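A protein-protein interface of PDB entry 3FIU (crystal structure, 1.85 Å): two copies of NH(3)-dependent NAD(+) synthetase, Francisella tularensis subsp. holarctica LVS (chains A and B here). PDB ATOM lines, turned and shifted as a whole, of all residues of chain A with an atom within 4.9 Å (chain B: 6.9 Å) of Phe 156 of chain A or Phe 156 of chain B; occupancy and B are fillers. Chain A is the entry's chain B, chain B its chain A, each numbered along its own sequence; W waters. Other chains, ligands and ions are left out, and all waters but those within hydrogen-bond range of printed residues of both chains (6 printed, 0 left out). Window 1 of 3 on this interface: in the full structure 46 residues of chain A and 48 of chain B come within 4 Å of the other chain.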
ATOM      1  N   ARG A 122      -4.344   9.171 -10.188  1.00  0.00           N
ATOM      2  CA  ARG A 122      -3.807   8.656 -11.451  1.00  0.00           C
ATOM      3  C   ARG A 122      -4.913   8.004 -12.270  1.00  0.00           C
ATOM      4  O   ARG A 122      -4.929   8.122 -13.495  1.00  0.00           O
ATOM      5  CB  ARG A 122      -2.674   7.655 -11.146  1.00  0.00           C
ATOM      6  CG  ARG A 122      -1.413   8.416 -10.700  1.00  0.00           C
ATOM      7  CD  ARG A 122      -0.298   7.533 -10.083  1.00  0.00           C
ATOM      8  NE  ARG A 122       0.744   8.451  -9.571  1.00  0.00           N
ATOM      9  CZ  ARG A 122       1.439   8.260  -8.445  1.00  0.00           C
ATOM     10  NH1 ARG A 122       1.207   7.178  -7.701  1.00  0.00           N
ATOM     11  NH2 ARG A 122       2.359   9.148  -8.062  1.00  0.00           N
ATOM     12  N   MET A 125      -6.607  10.812 -14.106  1.00  0.00           N
ATOM     13  CA  MET A 125      -5.759  11.106 -15.268  1.00  0.00           C
ATOM     14  C   MET A 125      -6.055  10.128 -16.424  1.00  0.00           C
ATOM     15  O   MET A 125      -6.151  10.537 -17.568  1.00  0.00           O
ATOM     16  CB  MET A 125      -4.286  11.058 -14.869  1.00  0.00           C
ATOM     17  CG  MET A 125      -3.281  11.295 -15.981  1.00  0.00           C
ATOM     18  SD  MET A 125      -2.941   9.846 -17.002  1.00  0.00           S
ATOM     19  CE  MET A 125      -2.100   8.721 -15.845  1.00  0.00           C
ATOM     20  N   TYR A 129      -7.462  11.333 -20.058  1.00  0.00           N
ATOM     21  CA  TYR A 129      -6.665  11.102 -21.288  1.00  0.00           C
ATOM     22  C   TYR A 129      -7.322  10.084 -22.197  1.00  0.00           C
ATOM     23  O   TYR A 129      -7.139  10.142 -23.421  1.00  0.00           O
ATOM     24  CB  TYR A 129      -5.204  10.707 -20.980  1.00  0.00           C
ATOM     25  CG  TYR A 129      -4.393  11.951 -20.756  1.00  0.00           C
ATOM     26  CD1 TYR A 129      -4.207  12.457 -19.475  1.00  0.00           C
ATOM     27  CD2 TYR A 129      -3.889  12.682 -21.848  1.00  0.00           C
ATOM     28  CE1 TYR A 129      -3.503  13.645 -19.274  1.00  0.00           C
ATOM     29  CE2 TYR A 129      -3.175  13.860 -21.657  1.00  0.00           C
ATOM     30  CZ  TYR A 129      -2.994  14.329 -20.365  1.00  0.00           C
ATOM     31  OH  TYR A 129      -2.299  15.507 -20.182  1.00  0.00           O
ATOM     32  N   THR A 154      -0.685  15.118  -7.169  1.00  0.00           N
ATOM     33  CA  THR A 154      -0.095  13.801  -7.385  1.00  0.00           C
ATOM     34  C   THR A 154       0.711  13.823  -8.678  1.00  0.00           C
ATOM     35  O   THR A 154       0.216  14.241  -9.721  1.00  0.00           O
ATOM     36  CB  THR A 154      -1.226  12.731  -7.485  1.00  0.00           C
ATOM     37  OG1 THR A 154      -1.921  12.650  -6.234  1.00  0.00           O
ATOM     38  CG2 THR A 154      -0.663  11.345  -7.873  1.00  0.00           C
ATOM     39  N   LYS A 155       1.971  13.392  -8.604  1.00  0.00           N
ATOM     40  CA  LYS A 155       2.801  13.232  -9.792  1.00  0.00           C
ATOM     41  C   LYS A 155       2.135  12.221 -10.727  1.00  0.00           C
ATOM     42  O   LYS A 155       1.842  11.106 -10.301  1.00  0.00           O
ATOM     43  CB  LYS A 155       4.171  12.659  -9.399  1.00  0.00           C
ATOM     44  CG  LYS A 155       5.233  12.804 -10.496  1.00  0.00           C
ATOM     45  CD  LYS A 155       6.632  12.420  -9.936  1.00  0.00           C
ATOM     46  CE  LYS A 155       7.722  12.759 -10.948  1.00  0.00           C
ATOM     47  NZ  LYS A 155       9.090  12.404 -10.420  1.00  0.00           N
ATOM     48  N   PHE A 156       1.906  12.632 -11.974  1.00  0.00           N
ATOM     49  CA  PHE A 156       1.228  11.837 -13.004  1.00  0.00           C
ATOM     50  C   PHE A 156      -0.241  11.563 -12.688  1.00  0.00           C
ATOM     51  O   PHE A 156      -0.882  10.706 -13.325  1.00  0.00           O
ATOM     52  CB  PHE A 156       2.027  10.541 -13.297  1.00  0.00           C
ATOM     53  CG  PHE A 156       3.472  10.799 -13.596  1.00  0.00           C
ATOM     54  CD1 PHE A 156       3.843  11.796 -14.500  1.00  0.00           C
ATOM     55  CD2 PHE A 156       4.470  10.064 -12.975  1.00  0.00           C
ATOM     56  CE1 PHE A 156       5.200  12.054 -14.772  1.00  0.00           C
ATOM     57  CE2 PHE A 156       5.822  10.320 -13.246  1.00  0.00           C
ATOM     58  CZ  PHE A 156       6.187  11.309 -14.138  1.00  0.00           C
ATOM     59  N   GLY A 157      -0.767  12.304 -11.709  1.00  0.00           N
ATOM     60  CA  GLY A 157      -2.179  12.258 -11.356  1.00  0.00           C
ATOM     61  C   GLY A 157      -2.814  13.596 -11.762  1.00  0.00           C
ATOM     62  O   GLY A 157      -2.868  13.927 -12.945  1.00  0.00           O
ATOM     63  N   ASP A 158      -3.269  14.379 -10.791  1.00  0.00           N
ATOM     64  CA  ASP A 158      -3.793  15.702 -11.121  1.00  0.00           C
ATOM     65  C   ASP A 158      -2.671  16.645 -11.581  1.00  0.00           C
ATOM     66  O   ASP A 158      -2.939  17.671 -12.212  1.00  0.00           O
ATOM     67  CB  ASP A 158      -4.597  16.315  -9.972  1.00  0.00           C
ATOM     68  CG  ASP A 158      -3.792  16.430  -8.676  1.00  0.00           C
ATOM     69  OD1 ASP A 158      -3.841  17.512  -8.080  1.00  0.00           O
ATOM     70  OD2 ASP A 158      -3.181  15.425  -8.237  1.00  0.00           O
ATOM     71  N   GLY A 159      -1.421  16.280 -11.281  1.00  0.00           N
ATOM     72  CA  GLY A 159      -0.261  17.036 -11.783  1.00  0.00           C
ATOM     73  C   GLY A 159       0.021  16.791 -13.266  1.00  0.00           C
ATOM     74  O   GLY A 159       0.862  17.476 -13.863  1.00  0.00           O
ATOM     75  N   ALA A 160      -0.667  15.821 -13.862  1.00  0.00           N
ATOM     76  CA  ALA A 160      -0.475  15.465 -15.280  1.00  0.00           C
ATOM     77  C   ALA A 160      -1.541  16.124 -16.145  1.00  0.00           C
ATOM     78  O   ALA A 160      -2.724  15.788 -16.055  1.00  0.00           O
ATOM     79  CB  ALA A 160      -0.530  13.942 -15.463  1.00  0.00           C
ATOM     80  N   ALA A 161      -1.122  17.048 -16.998  1.00  0.00           N
ATOM     81  CA  ALA A 161      -2.075  17.728 -17.876  1.00  0.00           C
ATOM     82  C   ALA A 161      -1.363  18.283 -19.107  1.00  0.00           C
ATOM     83  O   ALA A 161      -0.140  18.236 -19.175  1.00  0.00           O
ATOM     84  CB  ALA A 161      -2.806  18.832 -17.099  1.00  0.00           C
ATOM     85  N   ASP A 162      -2.132  18.798 -20.070  1.00  0.00           N
ATOM     86  CA  ASP A 162      -1.563  19.365 -21.275  1.00  0.00           C
ATOM     87  C   ASP A 162      -1.352  20.880 -21.114  1.00  0.00           C
ATOM     88  O   ASP A 162      -0.430  21.463 -21.707  1.00  0.00           O
ATOM     89  CB  ASP A 162      -2.442  19.047 -22.481  1.00  0.00           C
ATOM     90  CG  ASP A 162      -2.595  17.545 -22.718  1.00  0.00           C
ATOM     91  OD1 ASP A 162      -1.618  16.785 -22.462  1.00  0.00           O
ATOM     92  OD2 ASP A 162      -3.686  17.122 -23.175  1.00  0.00           O
ATOM     93  N   ASN B 118      -2.518   2.690 -24.564  1.00  0.00           N
ATOM     94  CA  ASN B 118      -2.177   3.810 -23.678  1.00  0.00           C
ATOM     95  C   ASN B 118      -2.704   3.621 -22.250  1.00  0.00           C
ATOM     96  O   ASN B 118      -2.019   3.966 -21.281  1.00  0.00           O
ATOM     97  CB  ASN B 118      -2.694   5.121 -24.246  1.00  0.00           C
ATOM     98  CG  ASN B 118      -1.867   5.629 -25.421  1.00  0.00           C
ATOM     99  OD1 ASN B 118      -0.728   5.214 -25.634  1.00  0.00           O
ATOM    100  ND2 ASN B 118      -2.442   6.546 -26.178  1.00  0.00           N
ATOM    101  N   ALA B 121      -0.501   1.148 -20.494  1.00  0.00           N
ATOM    102  CA  ALA B 121       0.792   1.729 -20.098  1.00  0.00           C
ATOM    103  C   ALA B 121       0.668   2.586 -18.833  1.00  0.00           C
ATOM    104  O   ALA B 121       1.546   2.610 -18.012  1.00  0.00           O
ATOM    105  CB  ALA B 121       1.368   2.582 -21.237  1.00  0.00           C
ATOM    106  N   ARG B 122      -0.444   3.292 -18.697  1.00  0.00           N
ATOM    107  CA  ARG B 122      -0.685   4.129 -17.547  1.00  0.00           C
ATOM    108  C   ARG B 122      -1.020   3.265 -16.318  1.00  0.00           C
ATOM    109  O   ARG B 122      -0.659   3.618 -15.224  1.00  0.00           O
ATOM    110  CB  ARG B 122      -1.839   5.078 -17.861  1.00  0.00           C
ATOM    111  CG  ARG B 122      -1.415   6.100 -18.953  1.00  0.00           C
ATOM    112  CD  ARG B 122      -2.572   7.009 -19.358  1.00  0.00           C
ATOM    113  NE  ARG B 122      -2.048   7.939 -20.377  1.00  0.00           N
ATOM    114  CZ  ARG B 122      -2.600   8.187 -21.556  1.00  0.00           C
ATOM    115  NH1 ARG B 122      -3.787   7.668 -21.860  1.00  0.00           N
ATOM    116  NH2 ARG B 122      -1.973   9.017 -22.409  1.00  0.00           N
ATOM    117  N   LEU B 123      -1.718   2.159 -16.513  1.00  0.00           N
ATOM    118  CA  LEU B 123      -1.855   1.204 -15.406  1.00  0.00           C
ATOM    119  C   LEU B 123      -0.494   0.726 -14.890  1.00  0.00           C
ATOM    120  O   LEU B 123      -0.261   0.660 -13.670  1.00  0.00           O
ATOM    121  CB  LEU B 123      -2.684  -0.006 -15.809  1.00  0.00           C
ATOM    122  CG  LEU B 123      -4.193   0.158 -15.749  1.00  0.00           C
ATOM    123  CD1 LEU B 123      -4.820  -1.118 -16.267  1.00  0.00           C
ATOM    124  CD2 LEU B 123      -4.652   0.457 -14.312  1.00  0.00           C
ATOM    125  N   MET B 125       2.319   2.327 -15.019  1.00  0.00           N
ATOM    126  CA  MET B 125       2.830   3.493 -14.272  1.00  0.00           C
ATOM    127  C   MET B 125       2.282   3.495 -12.845  1.00  0.00           C
ATOM    128  O   MET B 125       3.049   3.709 -11.872  1.00  0.00           O
ATOM    129  CB  MET B 125       2.490   4.801 -15.012  1.00  0.00           C
ATOM    130  CG  MET B 125       2.983   6.105 -14.308  1.00  0.00           C
ATOM    131  SD  MET B 125       1.863   6.614 -13.006  1.00  0.00           S
ATOM    132  CE  MET B 125       0.438   7.262 -13.907  1.00  0.00           C
ATOM    133  N   MET B 126       0.994   3.197 -12.713  1.00  0.00           N
ATOM    134  CA  MET B 126       0.340   3.169 -11.399  1.00  0.00           C
ATOM    135  C   MET B 126       0.966   2.095 -10.504  1.00  0.00           C
ATOM    136  O   MET B 126       1.285   2.354  -9.354  1.00  0.00           O
ATOM    137  CB  MET B 126      -1.158   2.898 -11.543  1.00  0.00           C
ATOM    138  CG  MET B 126      -1.952   4.122 -12.073  1.00  0.00           C
ATOM    139  SD  MET B 126      -3.723   3.879 -12.110  1.00  0.00           S
ATOM    140  CE  MET B 126      -4.074   3.438 -10.402  1.00  0.00           C
ATOM    141  N   TYR B 129       4.579   3.212  -9.388  1.00  0.00           N
ATOM    142  CA  TYR B 129       4.478   4.265  -8.375  1.00  0.00           C
ATOM    143  C   TYR B 129       3.855   3.804  -7.048  1.00  0.00           C
ATOM    144  O   TYR B 129       4.233   4.299  -6.017  1.00  0.00           O
ATOM    145  CB  TYR B 129       3.759   5.514  -8.963  1.00  0.00           C
ATOM    146  CG  TYR B 129       4.783   6.339  -9.724  1.00  0.00           C
ATOM    147  CD1 TYR B 129       4.980   6.153 -11.105  1.00  0.00           C
ATOM    148  CD2 TYR B 129       5.665   7.185  -9.026  1.00  0.00           C
ATOM    149  CE1 TYR B 129       5.995   6.852 -11.785  1.00  0.00           C
ATOM    150  CE2 TYR B 129       6.646   7.884  -9.679  1.00  0.00           C
ATOM    151  CZ  TYR B 129       6.821   7.718 -11.060  1.00  0.00           C
ATOM    152  OH  TYR B 129       7.838   8.419 -11.704  1.00  0.00           O
ATOM    153  N   VAL B 139      11.351   5.365  -9.734  1.00  0.00           N
ATOM    154  CA  VAL B 139      10.905   4.595 -10.892  1.00  0.00           C
ATOM    155  C   VAL B 139      11.831   4.880 -12.058  1.00  0.00           C
ATOM    156  O   VAL B 139      11.950   6.030 -12.526  1.00  0.00           O
ATOM    157  CB  VAL B 139       9.438   4.971 -11.305  1.00  0.00           C
ATOM    158  CG1 VAL B 139       9.037   4.216 -12.584  1.00  0.00           C
ATOM    159  CG2 VAL B 139       8.490   4.679 -10.178  1.00  0.00           C
ATOM    160  N   PHE B 153       6.067   6.424 -27.103  1.00  0.00           N
ATOM    161  CA  PHE B 153       5.808   6.126 -25.703  1.00  0.00           C
ATOM    162  C   PHE B 153       4.476   6.766 -25.342  1.00  0.00           C
ATOM    163  O   PHE B 153       3.990   7.658 -26.047  1.00  0.00           O
ATOM    164  CB  PHE B 153       6.942   6.627 -24.786  1.00  0.00           C
ATOM    165  CG  PHE B 153       7.159   8.125 -24.818  1.00  0.00           C
ATOM    166  CD1 PHE B 153       6.377   8.986 -24.024  1.00  0.00           C
ATOM    167  CD2 PHE B 153       8.169   8.677 -25.607  1.00  0.00           C
ATOM    168  CE1 PHE B 153       6.596  10.385 -24.034  1.00  0.00           C
ATOM    169  CE2 PHE B 153       8.395  10.063 -25.633  1.00  0.00           C
ATOM    170  CZ  PHE B 153       7.592  10.923 -24.842  1.00  0.00           C
ATOM    171  N   THR B 154       3.863   6.275 -24.266  1.00  0.00           N
ATOM    172  CA  THR B 154       2.591   6.821 -23.806  1.00  0.00           C
ATOM    173  C   THR B 154       2.854   7.965 -22.845  1.00  0.00           C
ATOM    174  O   THR B 154       3.603   7.811 -21.855  1.00  0.00           O
ATOM    175  CB  THR B 154       1.770   5.727 -23.048  1.00  0.00           C
ATOM    176  OG1 THR B 154       1.528   4.607 -23.912  1.00  0.00           O
ATOM    177  CG2 THR B 154       0.413   6.313 -22.569  1.00  0.00           C
ATOM    178  N   LYS B 155       2.239   9.122 -23.102  1.00  0.00           N
ATOM    179  CA  LYS B 155       2.353  10.247 -22.178  1.00  0.00           C
ATOM    180  C   LYS B 155       1.732   9.847 -20.840  1.00  0.00           C
ATOM    181  O   LYS B 155       0.586   9.420 -20.816  1.00  0.00           O
ATOM    182  CB  LYS B 155       1.598  11.471 -22.723  1.00  0.00           C
ATOM    183  CG  LYS B 155       1.977  12.778 -22.052  1.00  0.00           C
ATOM    184  CD  LYS B 155       1.174  13.928 -22.701  1.00  0.00           C
ATOM    185  CE  LYS B 155       1.733  15.276 -22.286  1.00  0.00           C
ATOM    186  NZ  LYS B 155       1.056  16.418 -23.029  1.00  0.00           N
ATOM    187  N   PHE B 156       2.494  10.000 -19.755  1.00  0.00           N
ATOM    188  CA  PHE B 156       2.108   9.563 -18.389  1.00  0.00           C
ATOM    189  C   PHE B 156       1.885   8.050 -18.244  1.00  0.00           C
ATOM    190  O   PHE B 156       1.253   7.582 -17.260  1.00  0.00           O
ATOM    191  CB  PHE B 156       0.898  10.368 -17.855  1.00  0.00           C
ATOM    192  CG  PHE B 156       1.030  11.856 -18.084  1.00  0.00           C
ATOM    193  CD1 PHE B 156       2.127  12.562 -17.572  1.00  0.00           C
ATOM    194  CD2 PHE B 156       0.055  12.566 -18.801  1.00  0.00           C
ATOM    195  CE1 PHE B 156       2.269  13.942 -17.776  1.00  0.00           C
ATOM    196  CE2 PHE B 156       0.201  13.948 -19.012  1.00  0.00           C
ATOM    197  CZ  PHE B 156       1.307  14.631 -18.486  1.00  0.00           C
ATOM    198  N   GLY B 157       2.404   7.289 -19.209  1.00  0.00           N
ATOM    199  CA  GLY B 157       2.466   5.826 -19.092  1.00  0.00           C
ATOM    200  C   GLY B 157       3.941   5.468 -18.957  1.00  0.00           C
ATOM    201  O   GLY B 157       4.571   5.841 -17.988  1.00  0.00           O
ATOM    202  N   ASP B 158       4.511   4.811 -19.963  1.00  0.00           N
ATOM    203  CA  ASP B 158       5.938   4.472 -19.916  1.00  0.00           C
ATOM    204  C   ASP B 158       6.807   5.712 -20.085  1.00  0.00           C
ATOM    205  O   ASP B 158       7.967   5.703 -19.701  1.00  0.00           O
ATOM    206  CB  ASP B 158       6.292   3.365 -20.931  1.00  0.00           C
ATOM    207  CG  ASP B 158       5.967   3.751 -22.350  1.00  0.00           C
ATOM    208  OD1 ASP B 158       6.884   3.660 -23.179  1.00  0.00           O
ATOM    209  OD2 ASP B 158       4.814   4.152 -22.628  1.00  0.00           O
ATOM    210  N   GLY B 159       6.229   6.801 -20.609  1.00  0.00           N
ATOM    211  CA  GLY B 159       6.958   8.074 -20.679  1.00  0.00           C
ATOM    212  C   GLY B 159       7.072   8.769 -19.322  1.00  0.00           C
ATOM    213  O   GLY B 159       7.751   9.785 -19.195  1.00  0.00           O
ATOM    214  N   ALA B 160       6.421   8.220 -18.298  1.00  0.00           N
ATOM    215  CA  ALA B 160       6.378   8.834 -16.965  1.00  0.00           C
ATOM    216  C   ALA B 160       7.272   8.079 -16.002  1.00  0.00           C
ATOM    217  O   ALA B 160       6.971   6.939 -15.630  1.00  0.00           O
ATOM    218  CB  ALA B 160       4.959   8.842 -16.440  1.00  0.00           C
ATOM    219  N   ALA B 161       8.379   8.695 -15.593  1.00  0.00           N
ATOM    220  CA  ALA B 161       9.279   8.039 -14.650  1.00  0.00           C
ATOM    221  C   ALA B 161      10.026   9.102 -13.847  1.00  0.00           C
ATOM    222  O   ALA B 161       9.823  10.287 -14.073  1.00  0.00           O
ATOM    223  CB  ALA B 161      10.253   7.113 -15.398  1.00  0.00           C
ATOM    224  N   ASP B 162      10.861   8.673 -12.908  1.00  0.00           N
ATOM    225  CA  ASP B 162      11.641   9.608 -12.091  1.00  0.00           C
ATOM    226  C   ASP B 162      13.004   9.847 -12.708  1.00  0.00           C
ATOM    227  O   ASP B 162      13.602  10.911 -12.507  1.00  0.00           O
ATOM    228  CB  ASP B 162      11.802   9.078 -10.676  1.00  0.00           C
ATOM    229  CG  ASP B 162      10.477   8.923  -9.951  1.00  0.00           C
ATOM    230  OD1 ASP B 162       9.542   9.717 -10.226  1.00  0.00           O
ATOM    231  OD2 ASP B 162      10.373   8.020  -9.091  1.00  0.00           O
ATOM    232  N   LYS B 240       4.437  15.714 -26.028  1.00  0.00           N
ATOM    233  CA  LYS B 240       4.763  14.522 -25.215  1.00  0.00           C
ATOM    234  C   LYS B 240       6.083  14.630 -24.485  1.00  0.00           C
ATOM    235  O   LYS B 240       6.289  13.960 -23.480  1.00  0.00           O
ATOM    236  CB  LYS B 240       4.797  13.256 -26.072  1.00  0.00           C
ATOM    237  CG  LYS B 240       3.441  12.774 -26.464  1.00  0.00           C
ATOM    238  CD  LYS B 240       3.494  11.717 -27.550  1.00  0.00           C
ATOM    239  CE  LYS B 240       3.344  10.353 -26.978  1.00  0.00           C
ATOM    240  NZ  LYS B 240       2.945   9.396 -28.001  1.00  0.00           N
ATOM    241  N   LYS B 242       7.572  17.655 -23.435  1.00  0.00           N
ATOM    242  CA  LYS B 242       7.692  18.875 -22.609  1.00  0.00           C
ATOM    243  C   LYS B 242       6.691  18.928 -21.468  1.00  0.00           C
ATOM    244  O   LYS B 242       5.720  18.191 -21.456  1.00  0.00           O
ATOM    245  CB  LYS B 242       7.473  20.134 -23.474  1.00  0.00           C
ATOM    246  CG  LYS B 242       8.282  20.210 -24.773  1.00  0.00           C
ATOM    247  CD  LYS B 242       9.796  20.069 -24.539  1.00  0.00           C
ATOM    248  CE  LYS B 242      10.609  20.393 -25.809  1.00  0.00           C
ATOM    249  NZ  LYS B 242      11.714  19.399 -26.069  1.00  0.00           N
ATOM    250  N   ALA B 244       3.670  20.717 -19.288  1.00  0.00           N
ATOM    251  CA  ALA B 244       2.404  21.325 -19.688  1.00  0.00           C
ATOM    252  C   ALA B 244       2.572  22.809 -20.026  1.00  0.00           C
ATOM    253  O   ALA B 244       3.402  23.513 -19.389  1.00  0.00           O
ATOM    254  CB  ALA B 244       1.384  21.146 -18.570  1.00  0.00           C
HETATM  255  O   HOH W   1      -5.626   7.717 -24.209  1.00  0.00           O
HETATM  256  O   HOH W   2       1.960   5.992  -5.094  1.00  0.00           O
HETATM  257  O   HOH W   3      -0.254   4.571  -8.250  1.00  0.00           O
HETATM  258  O   HOH W   4       2.155  18.123 -21.182  1.00  0.00           O
HETATM  259  O   HOH W   5       9.989  12.821 -12.957  1.00  0.00           O
HETATM  260  O   HOH W   6      12.205  12.789 -10.973  1.00  0.00           O
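Printed residues of chain B within 4 Å of Arg 122 of chain A: Met 125 (3.7 Å), Met 126 (3.7 Å) and Tyr 129 (3.3 Å). Of the printed residues of chain B, Phe 156 of chain A touches Met 125, Tyr 129, Phe 156, Ala 160 and Ala 161. Of the printed residues of chain A, Met 126 of chain B touches Arg 122 (3.7 Å). Of chain A, only Met 125, Tyr 129, Phe 156, Ala 160 and Ala 161 come within 4 Å of Phe 156 of chain B. Of the printed residues of chain A, Ala 244 of chain B touches Ala 161 and Asp 162. The nearest residue of chain B that does not touch Phe 156 of chain A is Asp 162 of chain B (4.8 Å).
CD of Arg 122 of chain A touches SD of Met 125 of chain B (3.7 Å). Tyr 129 of chain B touches Arg 122 of chain A (CB to NH1, 3.3 Å). Met 125 of chain A touches Met 125 of chain B. Met 125 of chain A touches Phe 156 of chain B (CE to O, 3.8 Å). Phe 156 of chain A touches Met 125 of chain B (CB to CE, 3.7 Å). Phe 156 of chain A touches Tyr 129 of chain B. CZ of Phe 156 of chain A touches CB of Ala 160 of chain B, 3.6 Å away. Ala 160 of chain A touches Phe 156 of chain B. CZ of Phe 156 of chain B touches N of Ala 161 of chain A, at 3.7 Å. Ala 244 of chain B touches Asp 162 of chain A.
The side-chain carboxylate (OD1) of Asp 162 of chain A lies within salt-bridge range of the side-chain amino group (NZ) of Lys 155 of chain B (2.8 Å). OD1 of Asp 162 of chain B lies within salt-bridge range of NZ of Lys 155 of chain A, at 2.7 Å.
The guanidinium group (NH2) of Arg 122 of chain B is in hydrogen-bond range of the backbone carbonyl oxygen (O) of Lys 155 of chain B (3.0 Å). OH of Tyr 129 of chain B is in hydrogen-bond range of OD1 of Asp 162 of chain B. The backbone carbonyl oxygen (O) of Val 139 of chain B sits at hydrogen-bond distance from the backbone NH (N) of Asp 162 of chain B (2.9 Å). The backbone carbonyl oxygen (O) of Lys 155 of chain A is in hydrogen-bond range of the guanidinium group (NE) of Arg 122 of chain A (3.0 Å). The side-chain carboxylate of Asp 162 of chain A lies within hydrogen-bond range of the side-chain hydroxyl of Tyr 129 of chain A.
Hydrophobic or aromatic side chains of chain B that line the printed part of chain A: Met 125, Met 126, Tyr 129, Phe 156, Ala 160 and Ala 244. Of the 12 printed residues of chain A, 8 touch a printed residue of chain B. Among the printed residues, 19 pairs touch across the chains. Among the printed residues, Asp or Glu carboxylates within 4 Å of a Lys or Arg side-chain nitrogen of the other chain: Lys 155 of chain A with Asp 162 of chain B (2.7 Å) and Asp 162 of chain A with Lys 155 of chain B (2.8 Å).
Arg 122 of chain A touches Tyr 129 of chain B, and with the chains exchanged Tyr 129 of chain A touches Arg 122 of chain B. Met 125 of chain A touches Phe 156 of chain B, and with the chains exchanged Phe 156 of chain A touches Met 125 of chain B. Lys 155 of chain A touches Asp 162 of chain B, and with the chains exchanged Asp 162 of chain A touches Lys 155 of chain B. Phe 156 of chain A touches Ala 161 of chain B, and with the chains exchanged Ala 161 of chain A touches Phe 156 of chain B.
Water W5 lies within hydrogen-bond range of NZ of Lys 155 of chain A and O of Ala 161 of chain B. Water W4 bridges the side-chain amino group of Lys 155 of chain B and the backbone carbonyl oxygen of Ala 161 of chain A. Water W6 lies within hydrogen-bond range of O of Asp 162 of chain B and NZ of Lys 155 of chain A. Water W3 lies within hydrogen-bond range of the backbone carbonyl oxygen of Met 126 of chain B (2.9 Å) and the guanidinium group of Arg 122 of chain A (3.0 Å). Water W2 lies within hydrogen-bond range of NH1 of Arg 122 of chain A (3.0 Å) and O of Tyr 129 of chain B (3.0 Å). Water W1 lies within hydrogen-bond range of O of Tyr 129 of chain A (3.0 Å) and NH1 of Arg 122 of chain B (3.0 Å).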
